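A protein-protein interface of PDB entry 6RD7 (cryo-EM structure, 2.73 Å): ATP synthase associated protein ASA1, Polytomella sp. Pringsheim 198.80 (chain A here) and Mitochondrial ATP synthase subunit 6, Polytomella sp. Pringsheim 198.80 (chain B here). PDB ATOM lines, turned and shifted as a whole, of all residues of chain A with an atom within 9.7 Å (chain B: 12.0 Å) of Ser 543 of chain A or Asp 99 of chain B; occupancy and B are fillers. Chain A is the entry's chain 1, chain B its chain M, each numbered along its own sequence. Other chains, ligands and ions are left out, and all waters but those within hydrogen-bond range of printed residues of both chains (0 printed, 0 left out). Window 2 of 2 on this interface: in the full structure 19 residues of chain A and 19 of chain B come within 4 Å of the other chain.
Printed residues of chain B within 4 Å of Asp 539 of chain A: Lys 101. Of the printed residues of chain B, Leu 540 of chain A touches Val 100, Lys 101 and Thr 102. His 542 of chain A touches just these residues of chain B: Asp 99, Val 100 and Thr 102. Of chain B, only Asp 99 (2.4 Å) comes within 4 Å of Ser 543 of chain A. No residue of chain B comes within 4 Å of Val 544 of chain A. No residue of chain B comes within 4 Å of Val 545 of chain A. No residue of chain B comes within 4 Å of Ala 546 of chain A. No residue of chain B comes within 4 Å of His 547 of chain A. Of chain A, only Pro 541, His 542 and Ser 543 come within 4 Å of Asp 99 of chain B. Val 100 of chain B touches just these residues of chain A: Leu 540, Pro 541 and His 542. Of the printed residues of chain A, Thr 102 of chain B touches Leu 540 (2.8 Å) and His 542 (3.5 Å). The nearest residue of chain B that does not touch Ser 543 of chain A is Val 100 of chain B (5.0 Å).
Asp 539 of chain A touches Lys 101 of chain B. Leu 540 of chain A touches Val 100 of chain B. Leu 540 of chain A touches Lys 101 of chain B. Asp 99 of chain B touches Pro 541 of chain A. CA of Pro 541 of chain A touches O of Val 100 of chain B, 3.4 Å away. CD2 of His 542 of chain A touches CG2 of Thr 102 of chain B, 3.5 Å away.
The backbone NH (N) of His 542 of chain A lies within hydrogen-bond range of the backbone carbonyl oxygen (O) of Val 100 of chain B. The backbone carbonyl oxygen of Leu 540 of chain A sits at hydrogen-bond distance from the backbone NH of Thr 102 of chain B (2.8 Å). The side-chain carboxylate of Asp 99 of chain B lies within hydrogen-bond range of the backbone NH of His 542 of chain A, 3.3 Å away. The side-chain carboxylate (OD2) of Asp 99 of chain B sits at hydrogen-bond distance from the side-chain hydroxyl (OG) of Ser 543 of chain A (2.4 Å).
Of the 14 printed residues of chain A, 5 touch a printed residue of chain B. Hydrophobic or aromatic side chains of chain A that line the printed part of chain B: Leu 540, Pro 541 and His 542. Of the 13 printed residues of chain B, 4 touch a printed residue of chain A. Hydrophobic or aromatic side chains of chain B within 4 Å of the printed part of chain A: Val 100. Among the printed residues, no Asp or Glu carboxylate lies within 4 Å of a Lys or Arg side-chain nitrogen of the other chain.
O of Lys 101 of chain B is in hydrogen-bond range of OG of Ser 104 of chain B, 2.9 Å away.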
ATOM      1  N   HIS A 531      30.781  34.637  33.896  1.00  0.00           N
ATOM      2  CA  HIS A 531      29.326  34.569  33.800  1.00  0.00           C
ATOM      3  C   HIS A 531      28.834  33.132  33.673  1.00  0.00           C
ATOM      4  O   HIS A 531      27.827  32.761  34.300  1.00  0.00           O
ATOM      5  CB  HIS A 531      28.841  35.398  32.619  1.00  0.00           C
ATOM      6  CG  HIS A 531      27.353  35.523  32.544  1.00  0.00           C
ATOM      7  ND1 HIS A 531      26.633  36.339  33.385  1.00  0.00           N
ATOM      8  CD2 HIS A 531      26.451  34.936  31.726  1.00  0.00           C
ATOM      9  CE1 HIS A 531      25.351  36.251  33.088  1.00  0.00           C
ATOM     10  NE2 HIS A 531      25.213  35.407  32.084  1.00  0.00           N
ATOM     11  N   ASP A 539      20.678  28.569  36.546  1.00  0.00           N
ATOM     12  CA  ASP A 539      19.654  29.213  35.737  1.00  0.00           C
ATOM     13  C   ASP A 539      20.151  29.704  34.386  1.00  0.00           C
ATOM     14  O   ASP A 539      19.459  30.502  33.757  1.00  0.00           O
ATOM     15  CB  ASP A 539      19.016  30.379  36.500  1.00  0.00           C
ATOM     16  CG  ASP A 539      20.030  31.389  36.994  1.00  0.00           C
ATOM     17  OD1 ASP A 539      21.242  31.117  36.931  1.00  0.00           O
ATOM     18  OD2 ASP A 539      19.609  32.466  37.453  1.00  0.00           O
ATOM     19  N   LEU A 540      21.317  29.272  33.929  1.00  0.00           N
ATOM     20  CA  LEU A 540      21.858  29.771  32.666  1.00  0.00           C
ATOM     21  C   LEU A 540      21.041  29.247  31.498  1.00  0.00           C
ATOM     22  O   LEU A 540      20.835  28.034  31.396  1.00  0.00           O
ATOM     23  CB  LEU A 540      23.314  29.353  32.511  1.00  0.00           C
ATOM     24  CG  LEU A 540      24.202  30.023  31.463  1.00  0.00           C
ATOM     25  CD1 LEU A 540      24.054  31.525  31.484  1.00  0.00           C
ATOM     26  CD2 LEU A 540      25.632  29.641  31.722  1.00  0.00           C
ATOM     27  N   PRO A 541      20.527  30.104  30.625  1.00  0.00           N
ATOM     28  CA  PRO A 541      19.836  29.614  29.435  1.00  0.00           C
ATOM     29  C   PRO A 541      20.811  29.033  28.430  1.00  0.00           C
ATOM     30  O   PRO A 541      21.994  29.375  28.403  1.00  0.00           O
ATOM     31  CB  PRO A 541      19.160  30.872  28.878  1.00  0.00           C
ATOM     32  CG  PRO A 541      19.156  31.836  29.994  1.00  0.00           C
ATOM     33  CD  PRO A 541      20.390  31.559  30.764  1.00  0.00           C
ATOM     34  N   HIS A 542      20.296  28.134  27.596  1.00  0.00           N
ATOM     35  CA  HIS A 542      21.117  27.598  26.519  1.00  0.00           C
ATOM     36  C   HIS A 542      21.342  28.634  25.430  1.00  0.00           C
ATOM     37  O   HIS A 542      22.324  28.543  24.686  1.00  0.00           O
ATOM     38  CB  HIS A 542      20.469  26.346  25.937  1.00  0.00           C
ATOM     39  CG  HIS A 542      20.797  25.093  26.683  1.00  0.00           C
ATOM     40  ND1 HIS A 542      21.502  24.056  26.118  1.00  0.00           N
ATOM     41  CD2 HIS A 542      20.510  24.707  27.947  1.00  0.00           C
ATOM     42  CE1 HIS A 542      21.640  23.086  27.003  1.00  0.00           C
ATOM     43  NE2 HIS A 542      21.048  23.457  28.122  1.00  0.00           N
ATOM     44  N   SER A 543      20.454  29.624  25.327  1.00  0.00           N
ATOM     45  CA  SER A 543      20.623  30.684  24.342  1.00  0.00           C
ATOM     46  C   SER A 543      21.787  31.590  24.703  1.00  0.00           C
ATOM     47  O   SER A 543      22.532  32.032  23.827  1.00  0.00           O
ATOM     48  CB  SER A 543      19.340  31.496  24.227  1.00  0.00           C
ATOM     49  OG  SER A 543      18.869  31.880  25.500  1.00  0.00           O
ATOM     50  N   VAL A 544      21.969  31.859  25.995  1.00  0.00           N
ATOM     51  CA  VAL A 544      23.080  32.686  26.449  1.00  0.00           C
ATOM     52  C   VAL A 544      24.399  31.941  26.279  1.00  0.00           C
ATOM     53  O   VAL A 544      25.427  32.535  25.934  1.00  0.00           O
ATOM     54  CB  VAL A 544      22.823  33.116  27.905  1.00  0.00           C
ATOM     55  CG1 VAL A 544      23.924  33.982  28.432  1.00  0.00           C
ATOM     56  CG2 VAL A 544      21.520  33.866  27.985  1.00  0.00           C
ATOM     57  N   VAL A 545      24.372  30.621  26.468  1.00  0.00           N
ATOM     58  CA  VAL A 545      25.544  29.781  26.236  1.00  0.00           C
ATOM     59  C   VAL A 545      25.913  29.768  24.758  1.00  0.00           C
ATOM     60  O   VAL A 545      27.081  29.945  24.395  1.00  0.00           O
ATOM     61  CB  VAL A 545      25.273  28.362  26.770  1.00  0.00           C
ATOM     62  CG1 VAL A 545      26.232  27.366  26.183  1.00  0.00           C
ATOM     63  CG2 VAL A 545      25.365  28.341  28.265  1.00  0.00           C
ATOM     64  N   ALA A 546      24.921  29.589  23.884  1.00  0.00           N
ATOM     65  CA  ALA A 546      25.188  29.546  22.450  1.00  0.00           C
ATOM     66  C   ALA A 546      25.542  30.921  21.905  1.00  0.00           C
ATOM     67  O   ALA A 546      26.179  31.031  20.852  1.00  0.00           O
ATOM     68  CB  ALA A 546      23.984  28.971  21.714  1.00  0.00           C
ATOM     69  N   HIS A 547      25.129  31.979  22.598  1.00  0.00           N
ATOM     70  CA  HIS A 547      25.506  33.324  22.192  1.00  0.00           C
ATOM     71  C   HIS A 547      26.936  33.637  22.594  1.00  0.00           C
ATOM     72  O   HIS A 547      27.692  34.221  21.811  1.00  0.00           O
ATOM     73  CB  HIS A 547      24.543  34.335  22.805  1.00  0.00           C
ATOM     74  CG  HIS A 547      24.983  35.756  22.657  1.00  0.00           C
ATOM     75  ND1 HIS A 547      24.817  36.467  21.490  1.00  0.00           N
ATOM     76  CD2 HIS A 547      25.586  36.597  23.529  1.00  0.00           C
ATOM     77  CE1 HIS A 547      25.298  37.686  21.649  1.00  0.00           C
ATOM     78  NE2 HIS A 547      25.773  37.789  22.876  1.00  0.00           N
ATOM     79  N   MET A 548      27.326  33.255  23.810  1.00  0.00           N
ATOM     80  CA  MET A 548      28.657  33.590  24.302  1.00  0.00           C
ATOM     81  C   MET A 548      29.736  32.764  23.619  1.00  0.00           C
ATOM     82  O   MET A 548      30.787  33.295  23.247  1.00  0.00           O
ATOM     83  CB  MET A 548      28.719  33.387  25.808  1.00  0.00           C
ATOM     84  CG  MET A 548      28.261  34.570  26.599  1.00  0.00           C
ATOM     85  SD  MET A 548      28.754  34.360  28.298  1.00  0.00           S
ATOM     86  CE  MET A 548      27.489  33.231  28.816  1.00  0.00           C
ATOM     87  N   ASP A 549      29.509  31.468  23.453  1.00  0.00           N
ATOM     88  CA  ASP A 549      30.471  30.582  22.806  1.00  0.00           C
ATOM     89  C   ASP A 549      29.775  29.852  21.670  1.00  0.00           C
ATOM     90  O   ASP A 549      29.348  28.702  21.827  1.00  0.00           O
ATOM     91  CB  ASP A 549      31.079  29.600  23.806  1.00  0.00           C
ATOM     92  CG  ASP A 549      32.524  29.272  23.487  1.00  0.00           C
ATOM     93  OD1 ASP A 549      32.970  29.584  22.364  1.00  0.00           O
ATOM     94  OD2 ASP A 549      33.218  28.715  24.361  1.00  0.00           O
ATOM     95  N   PRO A 550      29.643  30.490  20.503  1.00  0.00           N
ATOM     96  CA  PRO A 550      28.987  29.816  19.378  1.00  0.00           C
ATOM     97  C   PRO A 550      29.822  28.721  18.750  1.00  0.00           C
ATOM     98  O   PRO A 550      29.251  27.778  18.191  1.00  0.00           O
ATOM     99  CB  PRO A 550      28.739  30.956  18.386  1.00  0.00           C
ATOM    100  CG  PRO A 550      29.770  31.944  18.696  1.00  0.00           C
ATOM    101  CD  PRO A 550      30.074  31.853  20.152  1.00  0.00           C
ATOM    102  N   ILE A 553      29.496  25.447  20.852  1.00  0.00           N
ATOM    103  CA  ILE A 553      28.194  24.860  20.567  1.00  0.00           C
ATOM    104  C   ILE A 553      28.176  24.259  19.167  1.00  0.00           C
ATOM    105  O   ILE A 553      27.582  23.201  18.946  1.00  0.00           O
ATOM    106  CB  ILE A 553      27.099  25.923  20.775  1.00  0.00           C
ATOM    107  CG1 ILE A 553      27.060  26.340  22.242  1.00  0.00           C
ATOM    108  CG2 ILE A 553      25.735  25.428  20.363  1.00  0.00           C
ATOM    109  CD1 ILE A 553      26.937  25.193  23.209  1.00  0.00           C
ATOM    110  N   SER B  95      10.306  26.512  13.437  1.00  0.00           N
ATOM    111  CA  SER B  95      11.629  26.919  12.975  1.00  0.00           C
ATOM    112  C   SER B  95      12.412  27.582  14.103  1.00  0.00           C
ATOM    113  O   SER B  95      13.635  27.707  14.035  1.00  0.00           O
ATOM    114  CB  SER B  95      11.512  27.864  11.779  1.00  0.00           C
ATOM    115  OG  SER B  95      10.911  27.211  10.676  1.00  0.00           O
ATOM    116  N   SER B  96      11.695  28.005  15.139  1.00  0.00           N
ATOM    117  CA  SER B  96      12.288  28.588  16.335  1.00  0.00           C
ATOM    118  C   SER B  96      12.261  27.550  17.446  1.00  0.00           C
ATOM    119  O   SER B  96      11.183  27.121  17.873  1.00  0.00           O
ATOM    120  CB  SER B  96      11.539  29.849  16.761  1.00  0.00           C
ATOM    121  OG  SER B  96      12.081  30.381  17.956  1.00  0.00           O
ATOM    122  N   VAL B  97      13.440  27.145  17.912  1.00  0.00           N
ATOM    123  CA  VAL B  97      13.502  26.175  18.992  1.00  0.00           C
ATOM    124  C   VAL B  97      13.372  26.889  20.329  1.00  0.00           C
ATOM    125  O   VAL B  97      13.670  28.084  20.460  1.00  0.00           O
ATOM    126  CB  VAL B  97      14.799  25.352  18.919  1.00  0.00           C
ATOM    127  CG1 VAL B  97      14.823  24.551  17.640  1.00  0.00           C
ATOM    128  CG2 VAL B  97      16.008  26.256  19.007  1.00  0.00           C
ATOM    129  N   ARG B  98      12.906  26.155  21.330  1.00  0.00           N
ATOM    130  CA  ARG B  98      12.680  26.743  22.639  1.00  0.00           C
ATOM    131  C   ARG B  98      13.991  26.876  23.399  1.00  0.00           C
ATOM    132  O   ARG B  98      14.996  26.242  23.072  1.00  0.00           O
ATOM    133  CB  ARG B  98      11.693  25.899  23.439  1.00  0.00           C
ATOM    134  CG  ARG B  98      12.228  24.548  23.859  1.00  0.00           C
ATOM    135  CD  ARG B  98      11.095  23.597  24.168  1.00  0.00           C
ATOM    136  NE  ARG B  98      10.175  23.473  23.043  1.00  0.00           N
ATOM    137  CZ  ARG B  98       9.009  22.844  23.101  1.00  0.00           C
ATOM    138  NH1 ARG B  98       8.617  22.279  24.230  1.00  0.00           N
ATOM    139  NH2 ARG B  98       8.235  22.780  22.030  1.00  0.00           N
ATOM    140  N   ASP B  99      13.974  27.723  24.420  1.00  0.00           N
ATOM    141  CA  ASP B  99      15.139  27.903  25.264  1.00  0.00           C
ATOM    142  C   ASP B  99      15.082  26.953  26.451  1.00  0.00           C
ATOM    143  O   ASP B  99      14.014  26.664  26.994  1.00  0.00           O
ATOM    144  CB  ASP B  99      15.231  29.346  25.748  1.00  0.00           C
ATOM    145  CG  ASP B  99      16.639  29.749  26.089  1.00  0.00           C
ATOM    146  OD1 ASP B  99      17.541  28.898  25.985  1.00  0.00           O
ATOM    147  OD2 ASP B  99      16.851  30.918  26.456  1.00  0.00           O
ATOM    148  N   VAL B 100      16.249  26.450  26.839  1.00  0.00           N
ATOM    149  CA  VAL B 100      16.361  25.460  27.898  1.00  0.00           C
ATOM    150  C   VAL B 100      17.235  26.038  29.002  1.00  0.00           C
ATOM    151  O   VAL B 100      18.241  26.699  28.738  1.00  0.00           O
ATOM    152  CB  VAL B 100      16.942  24.128  27.365  1.00  0.00           C
ATOM    153  CG1 VAL B 100      16.992  23.071  28.448  1.00  0.00           C
ATOM    154  CG2 VAL B 100      16.144  23.624  26.186  1.00  0.00           C
ATOM    155  N   LYS B 101      16.828  25.808  30.243  1.00  0.00           N
ATOM    156  CA  LYS B 101      17.627  26.134  31.412  1.00  0.00           C
ATOM    157  C   LYS B 101      18.642  25.026  31.643  1.00  0.00           C
ATOM    158  O   LYS B 101      18.288  23.846  31.612  1.00  0.00           O
ATOM    159  CB  LYS B 101      16.729  26.295  32.634  1.00  0.00           C
ATOM    160  CG  LYS B 101      17.429  26.721  33.891  1.00  0.00           C
ATOM    161  CD  LYS B 101      16.417  26.946  34.987  1.00  0.00           C
ATOM    162  CE  LYS B 101      15.905  25.633  35.524  1.00  0.00           C
ATOM    163  NZ  LYS B 101      16.979  24.890  36.227  1.00  0.00           N
ATOM    164  N   THR B 102      19.900  25.402  31.852  1.00  0.00           N
ATOM    165  CA  THR B 102      20.905  24.415  32.213  1.00  0.00           C
ATOM    166  C   THR B 102      20.657  23.919  33.628  1.00  0.00           C
ATOM    167  O   THR B 102      20.247  24.680  34.507  1.00  0.00           O
ATOM    168  CB  THR B 102      22.314  24.995  32.110  1.00  0.00           C
ATOM    169  OG1 THR B 102      22.424  26.141  32.957  1.00  0.00           O
ATOM    170  CG2 THR B 102      22.642  25.381  30.689  1.00  0.00           C
ATOM    171  N   GLY B 103      20.897  22.632  33.846  1.00  0.00           N
ATOM    172  CA  GLY B 103      20.706  22.069  35.162  1.00  0.00           C
ATOM    173  C   GLY B 103      19.282  21.728  35.509  1.00  0.00           C
ATOM    174  O   GLY B 103      18.965  21.592  36.693  1.00  0.00           O
ATOM    175  N   SER B 104      18.409  21.596  34.516  1.00  0.00           N
ATOM    176  CA  SER B 104      17.032  21.215  34.782  1.00  0.00           C
ATOM    177  C   SER B 104      16.969  19.762  35.218  1.00  0.00           C
ATOM    178  O   SER B 104      17.778  18.936  34.790  1.00  0.00           O
ATOM    179  CB  SER B 104      16.174  21.427  33.541  1.00  0.00           C
ATOM    180  OG  SER B 104      16.069  22.799  33.229  1.00  0.00           O
ATOM    181  N   LEU B 105      16.016  19.463  36.098  1.00  0.00           N
ATOM    182  CA  LEU B 105      15.793  18.099  36.577  1.00  0.00           C
ATOM    183  C   LEU B 105      15.486  17.074  35.481  1.00  0.00           C
ATOM    184  O   LEU B 105      16.008  15.950  35.581  1.00  0.00           O
ATOM    185  CB  LEU B 105      14.701  18.134  37.657  1.00  0.00           C
ATOM    186  CG  LEU B 105      14.346  16.849  38.399  1.00  0.00           C
ATOM    187  CD1 LEU B 105      14.196  17.129  39.870  1.00  0.00           C
ATOM    188  CD2 LEU B 105      13.068  16.239  37.863  1.00  0.00           C
ATOM    189  N   PRO B 106      14.670  17.354  34.439  1.00  0.00           N
ATOM    190  CA  PRO B 106      14.562  16.361  33.354  1.00  0.00           C
ATOM    191  C   PRO B 106      15.850  16.155  32.583  1.00  0.00           C
ATOM    192  O   PRO B 106      16.160  15.020  32.208  1.00  0.00           O
ATOM    193  CB  PRO B 106      13.461  16.942  32.462  1.00  0.00           C
ATOM    194  CG  PRO B 106      12.655  17.734  33.358  1.00  0.00           C
ATOM    195  CD  PRO B 106      13.631  18.390  34.253  1.00  0.00           C
ATOM    196  N   THR B 107      16.624  17.221  32.370  1.00  0.00           N
ATOM    197  CA  THR B 107      17.904  17.104  31.681  1.00  0.00           C
ATOM    198  C   THR B 107      18.899  16.288  32.493  1.00  0.00           C
ATOM    199  O   THR B 107      19.610  15.443  31.943  1.00  0.00           O
ATOM    200  CB  THR B 107      18.467  18.493  31.398  1.00  0.00           C
ATOM    201  OG1 THR B 107      17.446  19.312  30.820  1.00  0.00           O
ATOM    202  CG2 THR B 107      19.641  18.420  30.453  1.00  0.00           C
